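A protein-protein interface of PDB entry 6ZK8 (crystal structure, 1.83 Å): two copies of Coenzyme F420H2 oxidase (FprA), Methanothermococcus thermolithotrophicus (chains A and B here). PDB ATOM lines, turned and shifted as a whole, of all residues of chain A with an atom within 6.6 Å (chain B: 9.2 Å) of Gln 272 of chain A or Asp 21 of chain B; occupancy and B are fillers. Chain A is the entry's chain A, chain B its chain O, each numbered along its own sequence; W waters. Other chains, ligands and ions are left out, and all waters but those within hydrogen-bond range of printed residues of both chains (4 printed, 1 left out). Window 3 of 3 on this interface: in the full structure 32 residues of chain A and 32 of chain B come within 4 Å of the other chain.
OH of Tyr 264 of chain A lies within hydrogen-bond range of OD1 of Asp 21 of chain B (2.7 Å). The side-chain amide nitrogen (NE2) of Gln 272 of chain A sits at hydrogen-bond distance from the side-chain carboxylate (OD2) of Asp 21 of chain B (2.8 Å). A ring nitrogen (NE2) of His 276 of chain A lies within hydrogen-bond range of the side-chain carboxylate (OD2) of Asp 21 of chain B (2.9 Å). The backbone carbonyl oxygen of Asp 21 of chain B lies within hydrogen-bond range of the side-chain amide nitrogen of Asn 296 of chain A, 3.4 Å away. The guanidinium group (NH1) of Arg 23 of chain B lies within salt-bridge range of the side-chain carboxylate (OD2) of Asp 297 of chain A (2.9 Å).
The side-chain hydroxyl of Tyr 264 of chain A lies within hydrogen-bond range of the side-chain amide nitrogen of Gln 272 of chain A (2.7 Å). The backbone NH (N) of Tyr 264 of chain A lies within hydrogen-bond range of the backbone carbonyl oxygen (O) of Tyr 292 of chain A (3.1 Å). The backbone NH of Phe 293 of chain A sits at hydrogen-bond distance from the side-chain carboxylate of Asp 297 of chain A (3.0 Å). NH2 of Arg 23 of chain B sits at hydrogen-bond distance from O of Trp 20 of chain B, at 3.0 Å. The backbone carbonyl oxygen (O) of Asp 21 of chain B lies close to the guanidinium group (NH2) of Arg 23 of chain B (3.5 Å). The backbone carbonyl oxygen (O) of Arg 23 of chain B is in hydrogen-bond range of the backbone NH (N) of Leu 30 of chain B (3.1 Å).
Among the printed residues, pairs that only touch across the chains: Met 291 of chain A with Trp 20 of chain B (3.5 Å), His 276 of chain A with Trp 20 of chain B (3.5 Å), Asn 296 of chain A with Arg 23 of chain B (3.5 Å), Phe 293 of chain A with Asp 21 of chain B (3.8 Å), Met 291 of chain A with Asp 21 of chain B (3.9 Å) and His 276 of chain A with Met 1 of chain B (3.9 Å).
No residue of chain B comes within 4 Å of Thr 271 of chain A. Gln 272 of chain A touches just one residue of chain B: Asp 21. No residue of chain B comes within 4 Å of Ala 275 of chain A. Of the printed residues of chain B, His 276 of chain A touches Met 1, Trp 20 and Asp 21. Of the printed residues of chain B, Asn 296 of chain A touches Asp 21 and Arg 23. Of the printed residues of chain A, Arg 23 of chain B touches Asn 296 and Asp 297. The nearest residue of chain A that does not touch Asp 21 of chain B is Tyr 292 of chain A (5.1 Å). The nearest printed residue of chain A that does not touch Arg 23 of chain B is Met 291 of chain A (4.2 Å).
Among the printed residues, 11 pairs touch across the chains.
No position is printed for both chains.
Water W3 bridges a ring nitrogen (ND1) of His 276 of chain A (2.7 Å) and the side-chain amide nitrogen of Gln 59 of chain B (2.9 Å). Water W1 bridges NE1 of Trp 20 of chain B (2.8 Å) and O of His 276 of chain A (3.0 Å). Water W2 lies within hydrogen-bond range of OD1 of Asp 297 of chain A (2.9 Å), OD1 of Asn 31 of chain B (3.0 Å) and NH1 of Arg 23 of chain B (3.2 Å). Water W4 bridges OD1 of Asp 297 of chain A and NE of Arg 23 of chain B.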
ATOM      1  N   TYR A 264     -33.110 -25.471 -23.787  1.00  0.00           N
ATOM      2  CA  TYR A 264     -33.826 -26.708 -23.544  1.00  0.00           C
ATOM      3  C   TYR A 264     -34.219 -26.795 -22.075  1.00  0.00           C
ATOM      4  O   TYR A 264     -33.682 -26.104 -21.200  1.00  0.00           O
ATOM      5  CB  TYR A 264     -32.959 -27.940 -23.950  1.00  0.00           C
ATOM      6  CG  TYR A 264     -31.863 -28.203 -22.959  1.00  0.00           C
ATOM      7  CD1 TYR A 264     -30.674 -27.530 -23.021  1.00  0.00           C
ATOM      8  CD2 TYR A 264     -32.060 -29.083 -21.905  1.00  0.00           C
ATOM      9  CE1 TYR A 264     -29.691 -27.702 -22.041  1.00  0.00           C
ATOM     10  CE2 TYR A 264     -31.086 -29.290 -20.953  1.00  0.00           C
ATOM     11  CZ  TYR A 264     -29.896 -28.599 -21.032  1.00  0.00           C
ATOM     12  OH  TYR A 264     -28.908 -28.801 -20.064  1.00  0.00           O
ATOM     13  N   ASP A 265     -35.147 -27.691 -21.812  1.00  0.00           N
ATOM     14  CA  ASP A 265     -35.394 -28.187 -20.463  1.00  0.00           C
ATOM     15  C   ASP A 265     -35.441 -29.711 -20.545  1.00  0.00           C
ATOM     16  O   ASP A 265     -35.541 -30.281 -21.633  1.00  0.00           O
ATOM     17  CB  ASP A 265     -36.679 -27.626 -19.865  1.00  0.00           C
ATOM     18  CG  ASP A 265     -36.561 -27.403 -18.339  1.00  0.00           C
ATOM     19  OD1 ASP A 265     -35.774 -28.120 -17.692  1.00  0.00           O
ATOM     20  OD2 ASP A 265     -37.247 -26.512 -17.797  1.00  0.00           O
ATOM     21  N   THR A 266     -35.336 -30.369 -19.393  1.00  0.00           N
ATOM     22  CA  THR A 266     -35.326 -31.823 -19.322  1.00  0.00           C
ATOM     23  C   THR A 266     -35.768 -32.236 -17.940  1.00  0.00           C
ATOM     24  O   THR A 266     -35.597 -31.486 -16.987  1.00  0.00           O
ATOM     25  CB  THR A 266     -33.939 -32.377 -19.618  1.00  0.00           C
ATOM     26  OG1 THR A 266     -34.045 -33.772 -19.890  1.00  0.00           O
ATOM     27  CG2 THR A 266     -32.987 -32.183 -18.457  1.00  0.00           C
ATOM     28  N   GLY A 269     -33.028 -36.091 -18.517  1.00  0.00           N
ATOM     29  CA  GLY A 269     -31.731 -35.859 -19.125  1.00  0.00           C
ATOM     30  C   GLY A 269     -31.643 -36.160 -20.608  1.00  0.00           C
ATOM     31  O   GLY A 269     -30.619 -35.853 -21.229  1.00  0.00           O
ATOM     32  N   SER A 270     -32.677 -36.752 -21.190  1.00  0.00           N
ATOM     33  CA  SER A 270     -32.594 -37.172 -22.584  1.00  0.00           C
ATOM     34  C   SER A 270     -32.587 -35.977 -23.524  1.00  0.00           C
ATOM     35  O   SER A 270     -31.798 -35.948 -24.476  1.00  0.00           O
ATOM     36  CB  SER A 270     -33.746 -38.116 -22.912  1.00  0.00           C
ATOM     37  OG  SER A 270     -33.580 -39.335 -22.197  1.00  0.00           O
ATOM     38  N   THR A 271     -33.450 -34.981 -23.280  1.00  0.00           N
ATOM     39  CA  THR A 271     -33.436 -33.775 -24.114  1.00  0.00           C
ATOM     40  C   THR A 271     -32.121 -33.023 -23.971  1.00  0.00           C
ATOM     41  O   THR A 271     -31.649 -32.406 -24.936  1.00  0.00           O
ATOM     42  CB  THR A 271     -34.631 -32.869 -23.770  1.00  0.00           C
ATOM     43  OG1 THR A 271     -35.839 -33.631 -23.971  1.00  0.00           O
ATOM     44  CG2 THR A 271     -34.661 -31.637 -24.614  1.00  0.00           C
ATOM     45  N   GLN A 272     -31.518 -33.076 -22.780  1.00  0.00           N
ATOM     46  CA  GLN A 272     -30.211 -32.457 -22.553  1.00  0.00           C
ATOM     47  C   GLN A 272     -29.130 -33.118 -23.393  1.00  0.00           C
ATOM     48  O   GLN A 272     -28.308 -32.430 -24.009  1.00  0.00           O
ATOM     49  CB  GLN A 272     -29.850 -32.536 -21.076  1.00  0.00           C
ATOM     50  CG  GLN A 272     -28.500 -32.015 -20.738  1.00  0.00           C
ATOM     51  CD  GLN A 272     -28.229 -32.070 -19.229  1.00  0.00           C
ATOM     52  OE1 GLN A 272     -28.095 -33.133 -18.645  1.00  0.00           O
ATOM     53  NE2 GLN A 272     -28.190 -30.915 -18.599  1.00  0.00           N
ATOM     54  N   LYS A 273     -29.128 -34.452 -23.454  1.00  0.00           N
ATOM     55  CA  LYS A 273     -28.165 -35.150 -24.299  1.00  0.00           C
ATOM     56  C   LYS A 273     -28.343 -34.770 -25.764  1.00  0.00           C
ATOM     57  O   LYS A 273     -27.359 -34.611 -26.487  1.00  0.00           O
ATOM     58  CB  LYS A 273     -28.300 -36.662 -24.134  1.00  0.00           C
ATOM     59  CG  LYS A 273     -27.895 -37.184 -22.734  1.00  0.00           C
ATOM     60  CD  LYS A 273     -28.308 -38.640 -22.565  1.00  0.00           C
ATOM     61  CE  LYS A 273     -27.798 -39.209 -21.253  1.00  0.00           C
ATOM     62  NZ  LYS A 273     -28.665 -38.860 -20.102  1.00  0.00           N
ATOM     63  N   MET A 274     -29.592 -34.646 -26.229  1.00  0.00           N
ATOM     64  CA  MET A 274     -29.819 -34.192 -27.598  1.00  0.00           C
ATOM     65  C   MET A 274     -29.239 -32.791 -27.817  1.00  0.00           C
ATOM     66  O   MET A 274     -28.542 -32.550 -28.809  1.00  0.00           O
ATOM     67  CB  MET A 274     -31.317 -34.198 -27.911  1.00  0.00           C
ATOM     68  CG  MET A 274     -31.963 -35.525 -27.769  1.00  0.00           C
ATOM     69  SD  MET A 274     -33.756 -35.544 -28.086  1.00  0.00           S
ATOM     70  CE  MET A 274     -33.835 -35.291 -29.845  1.00  0.00           C
ATOM     71  N   ALA A 275     -29.512 -31.859 -26.891  1.00  0.00           N
ATOM     72  CA  ALA A 275     -29.025 -30.490 -27.021  1.00  0.00           C
ATOM     73  C   ALA A 275     -27.514 -30.468 -27.116  1.00  0.00           C
ATOM     74  O   ALA A 275     -26.946 -29.791 -27.977  1.00  0.00           O
ATOM     75  CB  ALA A 275     -29.486 -29.636 -25.837  1.00  0.00           C
ATOM     76  N   HIS A 276     -26.837 -31.222 -26.250  1.00  0.00           N
ATOM     77  CA  HIS A 276     -25.383 -31.266 -26.330  1.00  0.00           C
ATOM     78  C   HIS A 276     -24.900 -31.880 -27.645  1.00  0.00           C
ATOM     79  O   HIS A 276     -23.851 -31.486 -28.167  1.00  0.00           O
ATOM     80  CB  HIS A 276     -24.821 -32.041 -25.150  1.00  0.00           C
ATOM     81  CG  HIS A 276     -25.042 -31.378 -23.831  1.00  0.00           C
ATOM     82  ND1 HIS A 276     -24.491 -31.857 -22.665  1.00  0.00           N
ATOM     83  CD2 HIS A 276     -25.734 -30.263 -23.492  1.00  0.00           C
ATOM     84  CE1 HIS A 276     -24.851 -31.079 -21.658  1.00  0.00           C
ATOM     85  NE2 HIS A 276     -25.598 -30.099 -22.132  1.00  0.00           N
ATOM     86  N   ALA A 277     -25.647 -32.844 -28.190  1.00  0.00           N
ATOM     87  CA  ALA A 277     -25.263 -33.463 -29.450  1.00  0.00           C
ATOM     88  C   ALA A 277     -25.452 -32.504 -30.624  1.00  0.00           C
ATOM     89  O   ALA A 277     -24.639 -32.495 -31.554  1.00  0.00           O
ATOM     90  CB  ALA A 277     -26.078 -34.750 -29.673  1.00  0.00           C
ATOM     91  N   MET A 291     -25.447 -22.224 -24.689  1.00  0.00           N
ATOM     92  CA  MET A 291     -26.297 -23.306 -24.199  1.00  0.00           C
ATOM     93  C   MET A 291     -27.018 -22.879 -22.936  1.00  0.00           C
ATOM     94  O   MET A 291     -26.375 -22.495 -21.945  1.00  0.00           O
ATOM     95  CB  MET A 291     -25.473 -24.559 -23.922  1.00  0.00           C
ATOM     96  CG  MET A 291     -26.267 -25.772 -23.456  1.00  0.00           C
ATOM     97  SD  MET A 291     -27.152 -26.579 -24.798  1.00  0.00           S
ATOM     98  CE  MET A 291     -25.781 -27.201 -25.792  1.00  0.00           C
ATOM     99  N   TYR A 292     -28.343 -22.969 -22.964  1.00  0.00           N
ATOM    100  CA  TYR A 292     -29.156 -22.526 -21.840  1.00  0.00           C
ATOM    101  C   TYR A 292     -30.108 -23.631 -21.423  1.00  0.00           C
ATOM    102  O   TYR A 292     -30.730 -24.272 -22.268  1.00  0.00           O
ATOM    103  CB  TYR A 292     -29.974 -21.273 -22.169  1.00  0.00           C
ATOM    104  CG  TYR A 292     -29.166 -20.018 -22.277  1.00  0.00           C
ATOM    105  CD1 TYR A 292     -28.827 -19.310 -21.151  1.00  0.00           C
ATOM    106  CD2 TYR A 292     -28.765 -19.533 -23.502  1.00  0.00           C
ATOM    107  CE1 TYR A 292     -28.089 -18.158 -21.234  1.00  0.00           C
ATOM    108  CE2 TYR A 292     -28.021 -18.368 -23.591  1.00  0.00           C
ATOM    109  CZ  TYR A 292     -27.693 -17.693 -22.447  1.00  0.00           C
ATOM    110  OH  TYR A 292     -26.959 -16.542 -22.501  1.00  0.00           O
ATOM    111  N   PHE A 293     -30.217 -23.825 -20.116  1.00  0.00           N
ATOM    112  CA  PHE A 293     -31.001 -24.874 -19.467  1.00  0.00           C
ATOM    113  C   PHE A 293     -32.062 -24.160 -18.640  1.00  0.00           C
ATOM    114  O   PHE A 293     -31.739 -23.479 -17.656  1.00  0.00           O
ATOM    115  CB  PHE A 293     -30.070 -25.749 -18.622  1.00  0.00           C
ATOM    116  CG  PHE A 293     -30.743 -26.812 -17.818  1.00  0.00           C
ATOM    117  CD1 PHE A 293     -31.915 -27.369 -18.206  1.00  0.00           C
ATOM    118  CD2 PHE A 293     -30.133 -27.285 -16.664  1.00  0.00           C
ATOM    119  CE1 PHE A 293     -32.492 -28.358 -17.453  1.00  0.00           C
ATOM    120  CE2 PHE A 293     -30.699 -28.306 -15.914  1.00  0.00           C
ATOM    121  CZ  PHE A 293     -31.884 -28.817 -16.282  1.00  0.00           C
ATOM    122  N   ASN A 296     -32.236 -23.719 -14.783  1.00  0.00           N
ATOM    123  CA  ASN A 296     -31.259 -22.886 -14.093  1.00  0.00           C
ATOM    124  C   ASN A 296     -31.203 -21.453 -14.619  1.00  0.00           C
ATOM    125  O   ASN A 296     -30.869 -20.538 -13.865  1.00  0.00           O
ATOM    126  CB  ASN A 296     -29.847 -23.488 -14.228  1.00  0.00           C
ATOM    127  CG  ASN A 296     -29.675 -24.769 -13.477  1.00  0.00           C
ATOM    128  OD1 ASN A 296     -30.480 -25.116 -12.629  1.00  0.00           O
ATOM    129  ND2 ASN A 296     -28.601 -25.477 -13.761  1.00  0.00           N
ATOM    130  N   ASP A 297     -31.457 -21.252 -15.905  1.00  0.00           N
ATOM    131  CA  ASP A 297     -31.240 -19.996 -16.597  1.00  0.00           C
ATOM    132  C   ASP A 297     -32.575 -19.296 -16.874  1.00  0.00           C
ATOM    133  O   ASP A 297     -33.666 -19.843 -16.690  1.00  0.00           O
ATOM    134  CB  ASP A 297     -30.462 -20.253 -17.893  1.00  0.00           C
ATOM    135  CG  ASP A 297     -29.113 -20.939 -17.651  1.00  0.00           C
ATOM    136  OD1 ASP A 297     -28.412 -20.508 -16.724  1.00  0.00           O
ATOM    137  OD2 ASP A 297     -28.753 -21.928 -18.349  1.00  0.00           O
ATOM    138  N   PHE A 351     -36.903 -29.838 -30.925  1.00  0.00           N
ATOM    139  CA  PHE A 351     -36.507 -31.202 -30.603  1.00  0.00           C
ATOM    140  C   PHE A 351     -36.951 -31.581 -29.195  1.00  0.00           C
ATOM    141  O   PHE A 351     -37.386 -30.742 -28.402  1.00  0.00           O
ATOM    142  CB  PHE A 351     -34.984 -31.373 -30.749  1.00  0.00           C
ATOM    143  CG  PHE A 351     -34.181 -30.578 -29.767  1.00  0.00           C
ATOM    144  CD1 PHE A 351     -33.949 -29.214 -29.961  1.00  0.00           C
ATOM    145  CD2 PHE A 351     -33.640 -31.190 -28.638  1.00  0.00           C
ATOM    146  CE1 PHE A 351     -33.199 -28.503 -29.059  1.00  0.00           C
ATOM    147  CE2 PHE A 351     -32.889 -30.470 -27.724  1.00  0.00           C
ATOM    148  CZ  PHE A 351     -32.665 -29.133 -27.932  1.00  0.00           C
ATOM    149  N   MET B   1     -21.529 -40.686 -27.773  1.00  0.00           N
ATOM    150  CA  MET B   1     -21.930 -39.494 -28.585  1.00  0.00           C
ATOM    151  C   MET B   1     -20.756 -39.040 -29.473  1.00  0.00           C
ATOM    152  O   MET B   1     -19.573 -39.199 -29.122  1.00  0.00           O
ATOM    153  CB  MET B   1     -22.423 -38.348 -27.707  1.00  0.00           C
ATOM    154  CG  MET B   1     -21.397 -37.631 -26.911  1.00  0.00           C
ATOM    155  SD  MET B   1     -22.089 -36.192 -26.028  1.00  0.00           S
ATOM    156  CE  MET B   1     -22.258 -34.975 -27.281  1.00  0.00           C
ATOM    157  N   VAL B  17     -14.220 -32.055 -21.743  1.00  0.00           N
ATOM    158  CA  VAL B  17     -15.667 -32.067 -21.606  1.00  0.00           C
ATOM    159  C   VAL B  17     -16.170 -30.657 -21.329  1.00  0.00           C
ATOM    160  O   VAL B  17     -15.642 -29.957 -20.459  1.00  0.00           O
ATOM    161  CB  VAL B  17     -16.100 -33.017 -20.480  1.00  0.00           C
ATOM    162  CG1 VAL B  17     -17.573 -32.850 -20.170  1.00  0.00           C
ATOM    163  CG2 VAL B  17     -15.762 -34.452 -20.828  1.00  0.00           C
ATOM    164  N   LEU B  18     -17.197 -30.255 -22.064  1.00  0.00           N
ATOM    165  CA  LEU B  18     -17.862 -28.979 -21.856  1.00  0.00           C
ATOM    166  C   LEU B  18     -19.051 -29.207 -20.933  1.00  0.00           C
ATOM    167  O   LEU B  18     -20.059 -29.788 -21.336  1.00  0.00           O
ATOM    168  CB  LEU B  18     -18.308 -28.382 -23.187  1.00  0.00           C
ATOM    169  CG  LEU B  18     -17.279 -28.265 -24.290  1.00  0.00           C
ATOM    170  CD1 LEU B  18     -17.950 -27.844 -25.616  1.00  0.00           C
ATOM    171  CD2 LEU B  18     -16.210 -27.276 -23.922  1.00  0.00           C
ATOM    172  N   ASP B  19     -18.934 -28.769 -19.687  1.00  0.00           N
ATOM    173  CA  ASP B  19     -20.043 -28.827 -18.740  1.00  0.00           C
ATOM    174  C   ASP B  19     -20.823 -27.522 -18.897  1.00  0.00           C
ATOM    175  O   ASP B  19     -20.608 -26.522 -18.194  1.00  0.00           O
ATOM    176  CB  ASP B  19     -19.536 -29.052 -17.319  1.00  0.00           C
ATOM    177  CG  ASP B  19     -20.650 -29.499 -16.363  1.00  0.00           C
ATOM    178  OD1 ASP B  19     -21.840 -29.347 -16.717  1.00  0.00           O
ATOM    179  OD2 ASP B  19     -20.341 -29.989 -15.249  1.00  0.00           O
ATOM    180  N   TRP B  20     -21.733 -27.542 -19.880  1.00  0.00           N
ATOM    181  CA  TRP B  20     -22.498 -26.354 -20.223  1.00  0.00           C
ATOM    182  C   TRP B  20     -23.332 -25.854 -19.061  1.00  0.00           C
ATOM    183  O   TRP B  20     -23.493 -24.643 -18.896  1.00  0.00           O
ATOM    184  CB  TRP B  20     -23.434 -26.621 -21.391  1.00  0.00           C
ATOM    185  CG  TRP B  20     -22.813 -27.064 -22.669  1.00  0.00           C
ATOM    186  CD1 TRP B  20     -22.736 -28.341 -23.136  1.00  0.00           C
ATOM    187  CD2 TRP B  20     -22.220 -26.234 -23.665  1.00  0.00           C
ATOM    188  NE1 TRP B  20     -22.155 -28.364 -24.385  1.00  0.00           N
ATOM    189  CE2 TRP B  20     -21.818 -27.082 -24.732  1.00  0.00           C
ATOM    190  CE3 TRP B  20     -22.021 -24.859 -23.786  1.00  0.00           C
ATOM    191  CZ2 TRP B  20     -21.193 -26.596 -25.879  1.00  0.00           C
ATOM    192  CZ3 TRP B  20     -21.402 -24.379 -24.933  1.00  0.00           C
ATOM    193  CH2 TRP B  20     -21.004 -25.247 -25.968  1.00  0.00           C
ATOM    194  N   ASP B  21     -23.899 -26.772 -18.284  1.00  0.00           N
ATOM    195  CA  ASP B  21     -25.052 -26.544 -17.432  1.00  0.00           C
ATOM    196  C   ASP B  21     -24.726 -26.376 -15.950  1.00  0.00           C
ATOM    197  O   ASP B  21     -25.578 -25.898 -15.209  1.00  0.00           O
ATOM    198  CB  ASP B  21     -26.034 -27.711 -17.590  1.00  0.00           C
ATOM    199  CG  ASP B  21     -26.345 -28.034 -19.061  1.00  0.00           C
ATOM    200  OD1 ASP B  21     -26.775 -27.153 -19.827  1.00  0.00           O
ATOM    201  OD2 ASP B  21     -26.132 -29.182 -19.474  1.00  0.00           O
ATOM    202  N   ILE B  22     -23.513 -26.692 -15.502  1.00  0.00           N
ATOM    203  CA  ILE B  22     -23.208 -26.577 -14.080  1.00  0.00           C
ATOM    204  C   ILE B  22     -23.217 -25.110 -13.661  1.00  0.00           C
ATOM    205  O   ILE B  22     -22.712 -24.223 -14.368  1.00  0.00           O
ATOM    206  CB  ILE B  22     -21.868 -27.258 -13.758  1.00  0.00           C
ATOM    207  CG1 ILE B  22     -21.611 -27.215 -12.252  1.00  0.00           C
ATOM    208  CG2 ILE B  22     -20.730 -26.574 -14.454  1.00  0.00           C
ATOM    209  CD1 ILE B  22     -20.393 -28.044 -11.796  1.00  0.00           C
ATOM    210  N   ARG B  23     -23.809 -24.845 -12.506  1.00  0.00           N
ATOM    211  CA  ARG B  23     -23.896 -23.497 -11.979  1.00  0.00           C
ATOM    212  C   ARG B  23     -23.266 -23.325 -10.602  1.00  0.00           C
ATOM    213  O   ARG B  23     -23.156 -22.192 -10.137  1.00  0.00           O
ATOM    214  CB  ARG B  23     -25.373 -23.060 -11.911  1.00  0.00           C
ATOM    215  CG  ARG B  23     -26.081 -23.032 -13.274  1.00  0.00           C
ATOM    216  CD  ARG B  23     -25.479 -21.939 -14.186  1.00  0.00           C
ATOM    217  NE  ARG B  23     -26.029 -21.996 -15.557  1.00  0.00           N
ATOM    218  CZ  ARG B  23     -25.387 -22.529 -16.617  1.00  0.00           C
ATOM    219  NH1 ARG B  23     -25.958 -22.562 -17.812  1.00  0.00           N
ATOM    220  NH2 ARG B  23     -24.151 -23.015 -16.511  1.00  0.00           N
ATOM    221  N   MET B  24     -22.847 -24.394  -9.943  1.00  0.00           N
ATOM    222  CA  MET B  24     -22.194 -24.276  -8.645  1.00  0.00           C
ATOM    223  C   MET B  24     -21.215 -25.432  -8.475  1.00  0.00           C
ATOM    224  O   MET B  24     -21.465 -26.535  -8.941  1.00  0.00           O
ATOM    225  CB  MET B  24     -23.186 -24.306  -7.465  1.00  0.00           C
ATOM    226  CG  MET B  24     -24.281 -23.267  -7.533  1.00  0.00           C
ATOM    227  SD  MET B  24     -24.991 -22.989  -5.926  1.00  0.00           S
ATOM    228  CE  MET B  24     -23.568 -22.268  -5.045  1.00  0.00           C
ATOM    229  N   LEU B  30     -20.842 -20.293 -10.982  1.00  0.00           N
ATOM    230  CA  LEU B  30     -20.287 -20.220 -12.331  1.00  0.00           C
ATOM    231  C   LEU B  30     -21.393 -20.446 -13.358  1.00  0.00           C
ATOM    232  O   LEU B  30     -22.530 -20.775 -13.023  1.00  0.00           O
ATOM    233  CB  LEU B  30     -19.147 -21.217 -12.512  1.00  0.00           C
ATOM    234  CG  LEU B  30     -19.437 -22.603 -11.981  1.00  0.00           C
ATOM    235  CD1 LEU B  30     -20.132 -23.413 -13.064  1.00  0.00           C
ATOM    236  CD2 LEU B  30     -18.139 -23.244 -11.614  1.00  0.00           C
ATOM    237  N   ASN B  31     -21.063 -20.174 -14.608  1.00  0.00           N
ATOM    238  CA  ASN B  31     -21.984 -20.354 -15.728  1.00  0.00           C
ATOM    239  C   ASN B  31     -21.355 -21.367 -16.674  1.00  0.00           C
ATOM    240  O   ASN B  31     -21.014 -21.048 -17.807  1.00  0.00           O
ATOM    241  CB  ASN B  31     -22.302 -19.036 -16.411  1.00  0.00           C
ATOM    242  CG  ASN B  31     -23.167 -18.142 -15.536  1.00  0.00           C
ATOM    243  OD1 ASN B  31     -24.415 -18.173 -15.609  1.00  0.00           O
ATOM    244  ND2 ASN B  31     -22.518 -17.362 -14.677  1.00  0.00           N
ATOM    245  N   GLY B  32     -21.197 -22.587 -16.171  1.00  0.00           N
ATOM    246  CA  GLY B  32     -20.571 -23.659 -16.888  1.00  0.00           C
ATOM    247  C   GLY B  32     -19.066 -23.647 -16.702  1.00  0.00           C
ATOM    248  O   GLY B  32     -18.453 -22.638 -16.341  1.00  0.00           O
ATOM    249  N   THR B  33     -18.465 -24.805 -16.964  1.00  0.00           N
ATOM    250  CA  THR B  33     -17.024 -24.880 -17.020  1.00  0.00           C
ATOM    251  C   THR B  33     -16.637 -26.018 -17.949  1.00  0.00           C
ATOM    252  O   THR B  33     -17.477 -26.605 -18.629  1.00  0.00           O
ATOM    253  CB  THR B  33     -16.465 -25.025 -15.601  1.00  0.00           C
ATOM    254  OG1 THR B  33     -15.049 -24.902 -15.634  1.00  0.00           O
ATOM    255  CG2 THR B  33     -16.829 -26.348 -15.027  1.00  0.00           C
ATOM    256  N   THR B  34     -15.352 -26.303 -18.011  1.00  0.00           N
ATOM    257  CA  THR B  34     -14.839 -27.438 -18.763  1.00  0.00           C
ATOM    258  C   THR B  34     -13.977 -28.290 -17.843  1.00  0.00           C
ATOM    259  O   THR B  34     -13.471 -27.819 -16.820  1.00  0.00           O
ATOM    260  CB  THR B  34     -14.019 -27.002 -19.973  1.00  0.00           C
ATOM    261  OG1 THR B  34     -12.797 -26.404 -19.523  1.00  0.00           O
ATOM    262  CG2 THR B  34     -14.789 -25.981 -20.819  1.00  0.00           C
ATOM    263  N   TYR B  35     -13.858 -29.567 -18.205  1.00  0.00           N
ATOM    264  CA  TYR B  35     -12.931 -30.513 -17.585  1.00  0.00           C
ATOM    265  C   TYR B  35     -11.984 -30.852 -18.716  1.00  0.00           C
ATOM    266  O   TYR B  35     -12.339 -31.640 -19.593  1.00  0.00           O
ATOM    267  CB  TYR B  35     -13.649 -31.753 -17.006  1.00  0.00           C
ATOM    268  CG  TYR B  35     -14.847 -31.339 -16.176  1.00  0.00           C
ATOM    269  CD1 TYR B  35     -14.688 -30.528 -15.062  1.00  0.00           C
ATOM    270  CD2 TYR B  35     -16.139 -31.716 -16.529  1.00  0.00           C
ATOM    271  CE1 TYR B  35     -15.771 -30.112 -14.341  1.00  0.00           C
ATOM    272  CE2 TYR B  35     -17.221 -31.317 -15.796  1.00  0.00           C
ATOM    273  CZ  TYR B  35     -17.039 -30.495 -14.712  1.00  0.00           C
ATOM    274  OH  TYR B  35     -18.107 -30.033 -13.960  1.00  0.00           O
ATOM    275  N   GLY B  55     -19.735 -39.565 -14.799  1.00  0.00           N
ATOM    276  CA  GLY B  55     -20.959 -39.470 -15.545  1.00  0.00           C
ATOM    277  C   GLY B  55     -20.927 -38.541 -16.723  1.00  0.00           C
ATOM    278  O   GLY B  55     -21.950 -38.443 -17.422  1.00  0.00           O
ATOM    279  N   THR B  56     -19.798 -37.861 -16.972  1.00  0.00           N
ATOM    280  CA  THR B  56     -19.683 -36.906 -18.072  1.00  0.00           C
ATOM    281  C   THR B  56     -18.703 -37.364 -19.151  1.00  0.00           C
ATOM    282  O   THR B  56     -18.271 -36.552 -19.964  1.00  0.00           O
ATOM    283  CB  THR B  56     -19.254 -35.532 -17.546  1.00  0.00           C
ATOM    284  OG1 THR B  56     -17.903 -35.610 -17.038  1.00  0.00           O
ATOM    285  CG2 THR B  56     -20.195 -35.056 -16.439  1.00  0.00           C
ATOM    286  N   GLN B  59     -18.667 -37.152 -23.869  1.00  0.00           N
ATOM    287  CA  GLN B  59     -17.944 -36.232 -24.744  1.00  0.00           C
ATOM    288  C   GLN B  59     -16.491 -36.647 -24.869  1.00  0.00           C
ATOM    289  O   GLN B  59     -15.928 -36.654 -25.971  1.00  0.00           O
ATOM    290  CB  GLN B  59     -18.020 -34.803 -24.210  1.00  0.00           C
ATOM    291  CG  GLN B  59     -19.316 -34.063 -24.494  1.00  0.00           C
ATOM    292  CD  GLN B  59     -19.303 -32.678 -23.909  1.00  0.00           C
ATOM    293  OE1 GLN B  59     -18.293 -31.989 -23.989  1.00  0.00           O
ATOM    294  NE2 GLN B  59     -20.401 -32.280 -23.267  1.00  0.00           N
ATOM    295  N   CYS B 178     -16.930 -21.791 -19.857  1.00  0.00           N
ATOM    296  CA  CYS B 178     -17.363 -22.817 -20.805  1.00  0.00           C
ATOM    297  C   CYS B 178     -17.702 -22.145 -22.129  1.00  0.00           C
ATOM    298  O   CYS B 178     -18.838 -21.708 -22.300  1.00  0.00           O
ATOM    299  CB  CYS B 178     -18.548 -23.594 -20.257  1.00  0.00           C
ATOM    300  SG  CYS B 178     -18.964 -25.038 -21.245  1.00  0.00           S
HETATM  301  O   HOH W   1     -21.790 -30.408 -26.262  1.00  0.00           O
HETATM  302  O   HOH W   2     -25.997 -19.374 -17.821  1.00  0.00           O
HETATM  303  O   HOH W   3     -22.734 -33.909 -22.970  1.00  0.00           O
HETATM  304  O   HOH W   4     -27.460 -19.401 -13.966  1.00  0.00           O
